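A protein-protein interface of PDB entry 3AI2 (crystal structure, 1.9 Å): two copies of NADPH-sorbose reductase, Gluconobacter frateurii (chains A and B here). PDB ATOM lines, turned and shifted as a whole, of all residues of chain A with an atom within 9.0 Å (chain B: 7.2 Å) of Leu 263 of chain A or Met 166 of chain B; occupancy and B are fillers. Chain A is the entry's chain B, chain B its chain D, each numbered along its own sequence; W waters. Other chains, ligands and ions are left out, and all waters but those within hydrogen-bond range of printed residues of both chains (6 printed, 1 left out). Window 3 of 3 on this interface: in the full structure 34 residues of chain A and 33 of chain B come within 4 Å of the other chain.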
ATOM      1  N   VAL A 148      28.162   5.890  18.806  1.00  0.00           N
ATOM      2  CA  VAL A 148      28.646   7.181  19.334  1.00  0.00           C
ATOM      3  C   VAL A 148      28.508   7.344  20.864  1.00  0.00           C
ATOM      4  O   VAL A 148      29.241   8.106  21.490  1.00  0.00           O
ATOM      5  CB  VAL A 148      27.924   8.387  18.696  1.00  0.00           C
ATOM      6  CG1 VAL A 148      27.899   8.288  17.151  1.00  0.00           C
ATOM      7  CG2 VAL A 148      26.528   8.475  19.236  1.00  0.00           C
ATOM      8  N   GLN A 149      27.565   6.636  21.450  1.00  0.00           N
ATOM      9  CA  GLN A 149      27.363   6.681  22.905  1.00  0.00           C
ATOM     10  C   GLN A 149      27.557   5.257  23.466  1.00  0.00           C
ATOM     11  O   GLN A 149      26.602   4.484  23.540  1.00  0.00           O
ATOM     12  CB  GLN A 149      25.922   7.164  23.185  1.00  0.00           C
ATOM     13  CG  GLN A 149      25.669   7.494  24.621  1.00  0.00           C
ATOM     14  CD  GLN A 149      24.265   8.103  24.792  1.00  0.00           C
ATOM     15  OE1 GLN A 149      24.086   9.315  24.688  1.00  0.00           O
ATOM     16  NE2 GLN A 149      23.290   7.271  24.963  1.00  0.00           N
ATOM     17  N   ALA A 252      23.945   9.616   9.242  1.00  0.00           N
ATOM     18  CA  ALA A 252      23.712   8.663  10.316  1.00  0.00           C
ATOM     19  C   ALA A 252      22.409   9.141  10.972  1.00  0.00           C
ATOM     20  O   ALA A 252      22.296  10.322  11.460  1.00  0.00           O
ATOM     21  CB  ALA A 252      24.845   8.671  11.315  1.00  0.00           C
ATOM     22  N   PHE A 254      19.516   8.566  13.776  1.00  0.00           N
ATOM     23  CA  PHE A 254      19.317   7.843  15.021  1.00  0.00           C
ATOM     24  C   PHE A 254      17.837   7.610  15.202  1.00  0.00           C
ATOM     25  O   PHE A 254      17.036   8.497  14.882  1.00  0.00           O
ATOM     26  CB  PHE A 254      19.841   8.658  16.198  1.00  0.00           C
ATOM     27  CG  PHE A 254      21.331   8.712  16.277  1.00  0.00           C
ATOM     28  CD1 PHE A 254      22.020   7.949  17.221  1.00  0.00           C
ATOM     29  CD2 PHE A 254      22.060   9.552  15.420  1.00  0.00           C
ATOM     30  CE1 PHE A 254      23.411   8.023  17.334  1.00  0.00           C
ATOM     31  CE2 PHE A 254      23.454   9.633  15.512  1.00  0.00           C
ATOM     32  CZ  PHE A 254      24.131   8.871  16.473  1.00  0.00           C
ATOM     33  N   ASP A 256      15.884   6.426  18.327  1.00  0.00           N
ATOM     34  CA  ASP A 256      16.339   6.014  19.672  1.00  0.00           C
ATOM     35  C   ASP A 256      15.509   6.492  20.839  1.00  0.00           C
ATOM     36  O   ASP A 256      15.951   6.402  21.980  1.00  0.00           O
ATOM     37  CB  ASP A 256      17.786   6.460  19.897  1.00  0.00           C
ATOM     38  CG  ASP A 256      17.938   7.997  19.908  1.00  0.00           C
ATOM     39  OD1 ASP A 256      16.960   8.740  20.208  1.00  0.00           O
ATOM     40  OD2 ASP A 256      19.051   8.459  19.612  1.00  0.00           O
ATOM     41  N   LEU A 260      19.872   9.285  22.833  1.00  0.00           N
ATOM     42  CA  LEU A 260      21.146   9.983  22.634  1.00  0.00           C
ATOM     43  C   LEU A 260      21.211  11.205  23.501  1.00  0.00           C
ATOM     44  O   LEU A 260      20.300  12.035  23.436  1.00  0.00           O
ATOM     45  CB  LEU A 260      21.325  10.446  21.166  1.00  0.00           C
ATOM     46  CG  LEU A 260      22.651  11.155  20.839  1.00  0.00           C
ATOM     47  CD1 LEU A 260      23.793  10.207  21.029  1.00  0.00           C
ATOM     48  CD2 LEU A 260      22.609  11.469  19.348  1.00  0.00           C
ATOM     49  N   LYS A 261      22.275  11.352  24.296  1.00  0.00           N
ATOM     50  CA  LYS A 261      22.259  12.358  25.352  1.00  0.00           C
ATOM     51  C   LYS A 261      22.796  13.697  24.868  1.00  0.00           C
ATOM     52  O   LYS A 261      22.647  14.727  25.558  1.00  0.00           O
ATOM     53  CB  LYS A 261      23.061  11.855  26.587  1.00  0.00           C
ATOM     54  CG  LYS A 261      22.239  10.978  27.617  1.00  0.00           C
ATOM     55  CD  LYS A 261      20.756  10.810  27.204  1.00  0.00           C
ATOM     56  CE  LYS A 261      19.947   9.847  28.133  1.00  0.00           C
ATOM     57  NZ  LYS A 261      20.053   8.403  27.661  1.00  0.00           N
ATOM     58  N   THR A 262      23.425  13.669  23.696  1.00  0.00           N
ATOM     59  CA  THR A 262      24.007  14.829  23.108  1.00  0.00           C
ATOM     60  C   THR A 262      23.341  15.209  21.803  1.00  0.00           C
ATOM     61  O   THR A 262      22.489  14.458  21.240  1.00  0.00           O
ATOM     62  CB  THR A 262      25.524  14.660  22.877  1.00  0.00           C
ATOM     63  OG1 THR A 262      25.741  13.644  21.895  1.00  0.00           O
ATOM     64  CG2 THR A 262      26.180  14.250  24.175  1.00  0.00           C
ATOM     65  N   LEU A 263      23.711  16.407  21.357  1.00  0.00           N
ATOM     66  CA  LEU A 263      23.157  17.048  20.162  1.00  0.00           C
ATOM     67  C   LEU A 263      23.419  16.279  18.901  1.00  0.00           C
ATOM     68  O   LEU A 263      22.492  15.757  18.249  1.00  0.00           O
ATOM     69  CB  LEU A 263      23.755  18.456  20.007  1.00  0.00           C
ATOM     70  CG  LEU A 263      22.781  19.499  20.482  1.00  0.00           C
ATOM     71  CD1 LEU A 263      23.200  20.849  19.926  1.00  0.00           C
ATOM     72  CD2 LEU A 263      21.391  19.129  20.041  1.00  0.00           C
ATOM     73  OXT LEU A 263      24.612  16.171  18.565  1.00  0.00           O
ATOM     74  N   ALA B 143      16.425  23.449  10.979  1.00  0.00           N
ATOM     75  CA  ALA B 143      17.563  24.273  11.296  1.00  0.00           C
ATOM     76  C   ALA B 143      18.399  24.441  10.005  1.00  0.00           C
ATOM     77  O   ALA B 143      18.026  25.243   9.113  1.00  0.00           O
ATOM     78  CB  ALA B 143      18.376  23.665  12.446  1.00  0.00           C
ATOM     79  N   ALA B 147      24.031  24.599  11.219  1.00  0.00           N
ATOM     80  CA  ALA B 147      23.917  24.489  12.672  1.00  0.00           C
ATOM     81  C   ALA B 147      25.076  23.717  13.287  1.00  0.00           C
ATOM     82  O   ALA B 147      25.308  23.804  14.506  1.00  0.00           O
ATOM     83  CB  ALA B 147      22.618  23.782  13.028  1.00  0.00           C
ATOM     84  N   VAL B 148      25.705  22.849  12.493  1.00  0.00           N
ATOM     85  CA  VAL B 148      26.864  22.085  12.993  1.00  0.00           C
ATOM     86  C   VAL B 148      28.083  22.387  12.161  1.00  0.00           C
ATOM     87  O   VAL B 148      29.158  22.407  12.701  1.00  0.00           O
ATOM     88  CB  VAL B 148      26.686  20.536  13.051  1.00  0.00           C
ATOM     89  CG1 VAL B 148      25.436  20.171  13.885  1.00  0.00           C
ATOM     90  CG2 VAL B 148      26.635  19.931  11.716  1.00  0.00           C
ATOM     91  N   THR B 160      22.687  31.297  15.363  1.00  0.00           N
ATOM     92  CA  THR B 160      21.276  31.217  15.715  1.00  0.00           C
ATOM     93  C   THR B 160      20.684  29.844  15.305  1.00  0.00           C
ATOM     94  O   THR B 160      19.800  29.311  15.978  1.00  0.00           O
ATOM     95  CB  THR B 160      20.424  32.408  15.129  1.00  0.00           C
ATOM     96  OG1 THR B 160      20.541  32.439  13.708  1.00  0.00           O
ATOM     97  CG2 THR B 160      20.845  33.755  15.731  1.00  0.00           C
ATOM     98  N   LYS B 161      21.162  29.255  14.218  1.00  0.00           N
ATOM     99  CA  LYS B 161      20.691  27.890  13.827  1.00  0.00           C
ATOM    100  C   LYS B 161      21.227  26.775  14.755  1.00  0.00           C
ATOM    101  O   LYS B 161      20.513  25.824  15.028  1.00  0.00           O
ATOM    102  CB  LYS B 161      21.008  27.577  12.351  1.00  0.00           C
ATOM    103  CG  LYS B 161      20.218  28.405  11.329  1.00  0.00           C
ATOM    104  CD  LYS B 161      18.723  27.981  11.348  1.00  0.00           C
ATOM    105  CE  LYS B 161      18.024  28.406  10.032  1.00  0.00           C
ATOM    106  NZ  LYS B 161      16.663  27.775   9.944  1.00  0.00           N
ATOM    107  N   ALA B 162      22.475  26.902  15.245  1.00  0.00           N
ATOM    108  CA  ALA B 162      22.990  26.012  16.259  1.00  0.00           C
ATOM    109  C   ALA B 162      22.144  26.122  17.543  1.00  0.00           C
ATOM    110  O   ALA B 162      21.838  25.128  18.213  1.00  0.00           O
ATOM    111  CB  ALA B 162      24.478  26.382  16.585  1.00  0.00           C
ATOM    112  N   ALA B 163      21.775  27.342  17.899  1.00  0.00           N
ATOM    113  CA  ALA B 163      20.879  27.539  19.022  1.00  0.00           C
ATOM    114  C   ALA B 163      19.526  26.847  18.862  1.00  0.00           C
ATOM    115  O   ALA B 163      19.039  26.225  19.811  1.00  0.00           O
ATOM    116  CB  ALA B 163      20.647  29.053  19.299  1.00  0.00           C
ATOM    117  N   LEU B 164      18.931  26.983  17.680  1.00  0.00           N
ATOM    118  CA  LEU B 164      17.701  26.295  17.331  1.00  0.00           C
ATOM    119  C   LEU B 164      17.872  24.766  17.451  1.00  0.00           C
ATOM    120  O   LEU B 164      17.001  24.071  18.009  1.00  0.00           O
ATOM    121  CB  LEU B 164      17.268  26.672  15.889  1.00  0.00           C
ATOM    122  CG  LEU B 164      15.947  26.017  15.419  1.00  0.00           C
ATOM    123  CD1 LEU B 164      14.739  26.261  16.402  1.00  0.00           C
ATOM    124  CD2 LEU B 164      15.608  26.523  14.030  1.00  0.00           C
ATOM    125  N   MET B 165      18.979  24.223  16.946  1.00  0.00           N
ATOM    126  CA  MET B 165      19.150  22.799  17.013  1.00  0.00           C
ATOM    127  C   MET B 165      19.173  22.356  18.482  1.00  0.00           C
ATOM    128  O   MET B 165      18.593  21.333  18.808  1.00  0.00           O
ATOM    129  CB  MET B 165      20.430  22.396  16.279  1.00  0.00           C
ATOM    130  CG  MET B 165      20.631  20.931  16.290  1.00  0.00           C
ATOM    131  SD  MET B 165      22.039  20.619  15.212  1.00  0.00           S
ATOM    132  CE  MET B 165      22.442  18.948  15.692  1.00  0.00           C
ATOM    133  N   MET B 166      19.786  23.155  19.382  1.00  0.00           N
ATOM    134  CA  MET B 166      19.783  22.800  20.803  1.00  0.00           C
ATOM    135  C   MET B 166      18.416  22.957  21.414  1.00  0.00           C
ATOM    136  O   MET B 166      17.971  22.079  22.192  1.00  0.00           O
ATOM    137  CB  MET B 166      20.827  23.610  21.622  1.00  0.00           C
ATOM    138  CG  MET B 166      20.783  23.317  23.151  1.00  0.00           C
ATOM    139  SD  MET B 166      21.076  21.549  23.586  1.00  0.00           S
ATOM    140  CE  MET B 166      22.860  21.491  23.630  1.00  0.00           C
ATOM    141  N   PHE B 167      17.731  24.058  21.060  1.00  0.00           N
ATOM    142  CA  PHE B 167      16.352  24.227  21.519  1.00  0.00           C
ATOM    143  C   PHE B 167      15.493  22.975  21.217  1.00  0.00           C
ATOM    144  O   PHE B 167      14.751  22.452  22.099  1.00  0.00           O
ATOM    145  CB  PHE B 167      15.687  25.475  20.938  1.00  0.00           C
ATOM    146  CG  PHE B 167      14.265  25.555  21.282  1.00  0.00           C
ATOM    147  CD1 PHE B 167      13.887  25.863  22.592  1.00  0.00           C
ATOM    148  CD2 PHE B 167      13.288  25.191  20.354  1.00  0.00           C
ATOM    149  CE1 PHE B 167      12.521  25.909  22.952  1.00  0.00           C
ATOM    150  CE2 PHE B 167      11.913  25.249  20.707  1.00  0.00           C
ATOM    151  CZ  PHE B 167      11.543  25.589  22.017  1.00  0.00           C
ATOM    152  N   SER B 168      15.652  22.462  20.003  1.00  0.00           N
ATOM    153  CA  SER B 168      14.821  21.342  19.494  1.00  0.00           C
ATOM    154  C   SER B 168      15.000  20.142  20.421  1.00  0.00           C
ATOM    155  O   SER B 168      14.038  19.509  20.874  1.00  0.00           O
ATOM    156  CB  SER B 168      15.267  20.971  18.059  1.00  0.00           C
ATOM    157  OG  SER B 168      14.426  19.926  17.543  1.00  0.00           O
ATOM    158  N   LYS B 169      16.263  19.845  20.729  1.00  0.00           N
ATOM    159  CA  LYS B 169      16.610  18.756  21.608  1.00  0.00           C
ATOM    160  C   LYS B 169      16.066  18.942  23.029  1.00  0.00           C
ATOM    161  O   LYS B 169      15.594  17.956  23.630  1.00  0.00           O
ATOM    162  CB  LYS B 169      18.132  18.650  21.661  1.00  0.00           C
ATOM    163  CG  LYS B 169      18.676  17.575  22.630  1.00  0.00           C
ATOM    164  CD  LYS B 169      18.231  16.211  22.247  1.00  0.00           C
ATOM    165  CE  LYS B 169      19.251  15.150  22.638  1.00  0.00           C
ATOM    166  NZ  LYS B 169      18.748  13.871  22.152  1.00  0.00           N
ATOM    167  N   THR B 170      16.148  20.160  23.573  1.00  0.00           N
ATOM    168  CA  THR B 170      15.680  20.409  24.950  1.00  0.00           C
ATOM    169  C   THR B 170      14.161  20.343  25.000  1.00  0.00           C
ATOM    170  O   THR B 170      13.595  19.877  26.002  1.00  0.00           O
ATOM    171  CB  THR B 170      16.188  21.733  25.559  1.00  0.00           C
ATOM    172  OG1 THR B 170      15.682  22.861  24.845  1.00  0.00           O
ATOM    173  CG2 THR B 170      17.732  21.807  25.564  1.00  0.00           C
ATOM    174  N   LEU B 171      13.497  20.804  23.926  1.00  0.00           N
ATOM    175  CA  LEU B 171      12.033  20.722  23.865  1.00  0.00           C
ATOM    176  C   LEU B 171      11.664  19.263  23.793  1.00  0.00           C
ATOM    177  O   LEU B 171      10.743  18.840  24.482  1.00  0.00           O
ATOM    178  CB  LEU B 171      11.424  21.499  22.664  1.00  0.00           C
ATOM    179  CG  LEU B 171       9.880  21.542  22.649  1.00  0.00           C
ATOM    180  CD1 LEU B 171       9.390  22.379  23.911  1.00  0.00           C
ATOM    181  CD2 LEU B 171       9.416  22.239  21.359  1.00  0.00           C
ATOM    182  N   ALA B 172      12.431  18.483  23.019  1.00  0.00           N
ATOM    183  CA  ALA B 172      12.148  17.068  22.889  1.00  0.00           C
ATOM    184  C   ALA B 172      11.963  16.342  24.239  1.00  0.00           C
ATOM    185  O   ALA B 172      11.031  15.528  24.384  1.00  0.00           O
ATOM    186  CB  ALA B 172      13.159  16.375  22.111  1.00  0.00           C
ATOM    187  N   CYS B 184      14.739  17.604  14.735  1.00  0.00           N
ATOM    188  CA  CYS B 184      15.301  18.670  13.982  1.00  0.00           C
ATOM    189  C   CYS B 184      15.677  18.089  12.663  1.00  0.00           C
ATOM    190  O   CYS B 184      16.137  16.909  12.581  1.00  0.00           O
ATOM    191  CB  CYS B 184      16.484  19.269  14.796  1.00  0.00           C
ATOM    192  SG  CYS B 184      17.504  20.473  13.855  1.00  0.00           S
ATOM    193  N   GLY B 250      13.977  13.773  19.809  1.00  0.00           N
ATOM    194  CA  GLY B 250      15.199  14.496  20.155  1.00  0.00           C
ATOM    195  C   GLY B 250      16.345  14.268  19.170  1.00  0.00           C
ATOM    196  O   GLY B 250      17.500  14.454  19.520  1.00  0.00           O
ATOM    197  N   SER B 251      16.035  13.872  17.947  1.00  0.00           N
ATOM    198  CA  SER B 251      17.068  13.630  16.960  1.00  0.00           C
ATOM    199  C   SER B 251      17.273  14.811  16.004  1.00  0.00           C
ATOM    200  O   SER B 251      16.402  15.701  15.882  1.00  0.00           O
ATOM    201  CB  SER B 251      16.813  12.297  16.199  1.00  0.00           C
ATOM    202  OG  SER B 251      16.817  11.193  17.133  1.00  0.00           O
ATOM    203  N   ALA B 252      18.443  14.808  15.368  1.00  0.00           N
ATOM    204  CA  ALA B 252      18.758  15.736  14.283  1.00  0.00           C
ATOM    205  C   ALA B 252      19.055  14.906  13.067  1.00  0.00           C
ATOM    206  O   ALA B 252      19.963  14.024  13.067  1.00  0.00           O
ATOM    207  CB  ALA B 252      19.959  16.630  14.644  1.00  0.00           C
ATOM    208  N   PHE B 254      20.019  14.827   9.113  1.00  0.00           N
ATOM    209  CA  PHE B 254      20.607  15.605   8.008  1.00  0.00           C
ATOM    210  C   PHE B 254      20.059  15.136   6.665  1.00  0.00           C
ATOM    211  O   PHE B 254      19.858  13.940   6.434  1.00  0.00           O
ATOM    212  CB  PHE B 254      22.149  15.534   8.023  1.00  0.00           C
ATOM    213  CG  PHE B 254      22.774  16.281   9.167  1.00  0.00           C
ATOM    214  CD1 PHE B 254      23.343  17.537   8.974  1.00  0.00           C
ATOM    215  CD2 PHE B 254      22.732  15.762  10.442  1.00  0.00           C
ATOM    216  CE1 PHE B 254      23.900  18.238   9.996  1.00  0.00           C
ATOM    217  CE2 PHE B 254      23.264  16.481  11.502  1.00  0.00           C
ATOM    218  CZ  PHE B 254      23.850  17.718  11.274  1.00  0.00           C
HETATM  219  O   HOH W   1      15.388   9.377  18.116  1.00  0.00           O
HETATM  220  O   HOH W   2      19.623  16.510  18.231  1.00  0.00           O
HETATM  221  O   HOH W   3      19.803  11.470  13.649  1.00  0.00           O
HETATM  222  O   HOH W   4      17.699  11.330  20.668  1.00  0.00           O
HETATM  223  O   HOH W   5      21.346  12.640  10.123  1.00  0.00           O
HETATM  224  O   HOH W   6      19.173  11.001  18.417  1.00  0.00           O
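The backbone carbonyl oxygen (O) of Leu 260 of chain A is in hydrogen-bond range of the side-chain amino group (NZ) of Lys 169 of chain B (2.7 Å).
The side-chain carboxylate of Asp 256 of chain A lies close to the backbone NH of Leu 260 of chain A, 3.4 Å away.
NZ of Lys 169 of chain B lies within hydrogen-bond range of O of Gly 250 of chain B (3.0 Å).
The backbone NH (N) of Cys 184 of chain B is in hydrogen-bond range of the backbone carbonyl oxygen (O) of Ser 251 of chain B, 2.8 Å away.
Among the printed residues, merely in contact across the chains: Phe 254 of chain A with Ser 251 of chain B (3.5 Å), Thr 262 of chain A with Lys 169 of chain B (3.6 Å), Leu 263 of chain A with Lys 169 of chain B (3.7 Å), Leu 263 of chain A with Met 166 of chain B (3.7 Å), Leu 263 of chain A with Met 165 of chain B (3.8 Å) and Asp 256 of chain A with Ser 251 of chain B (3.9 Å).
Printed residues of chain B within 4 Å of Phe 254 of chain A: Ser 251.
Of the printed residues of chain B, Asp 256 of chain A touches Ser 251 (3.9 Å).
Of the printed residues of chain B, Thr 262 of chain A touches Lys 169 (3.6 Å).
Of chain B, only Met 165 (3.8 Å), Met 166 (3.7 Å) and Lys 169 (3.7 Å) come within 4 Å of Leu 263 of chain A.
Met 165 of chain B touches just one residue of chain A: Leu 263 (3.8 Å).
Met 166 of chain B touches just one residue of chain A: Leu 263 (3.7 Å).
Ser 168 of chain B touches none of the printed residues of chain A.
Thr 170 of chain B touches none of the printed residues of chain A.
Of the 21 printed residues of chain B, 4 touch a printed residue of chain A.
Hydrophobic or aromatic side chains of chain B that line the printed part of chain A: Met 166.
Of the 9 printed residues of chain A, 5 touch a printed residue of chain B.
Printed residues of chain A that touch a printed residue of chain B: Phe 254, Asp 256, Leu 260, Thr 262 and Leu 263.
Among the printed residues, 7 pairs touch across the chains.
3 positions are printed for both chains.
Of the 7 pairs that touch across the chains among the printed residues, none has its exchanged pair printed and touching as well.
Water W1 bridges the side-chain hydroxyl of Ser 251 of chain B (2.5 Å) and the side-chain carboxylate of Asp 256 of chain A (2.7 Å).
Water W3 lies within hydrogen-bond range of the backbone carbonyl oxygen of Ala 252 of chain B (2.6 Å) and the backbone NH of Phe 254 of chain A (2.9 Å).
Water W6 lies within hydrogen-bond range of OG of Ser 251 of chain B and OD2 of Asp 256 of chain A.
Water W4 lies within hydrogen-bond range of the side-chain carboxylate (OD1) of Asp 256 of chain A, the side-chain amino group (NZ) of Lys 169 of chain B and the backbone carbonyl oxygen (O) of Gly 250 of chain B.
Water W5 bridges N of Phe 254 of chain B (2.8 Å) and O of Ala 252 of chain A (2.8 Å).
Water W2 lies within hydrogen-bond range of O of Leu 263 of chain A and O of Gly 250 of chain B.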
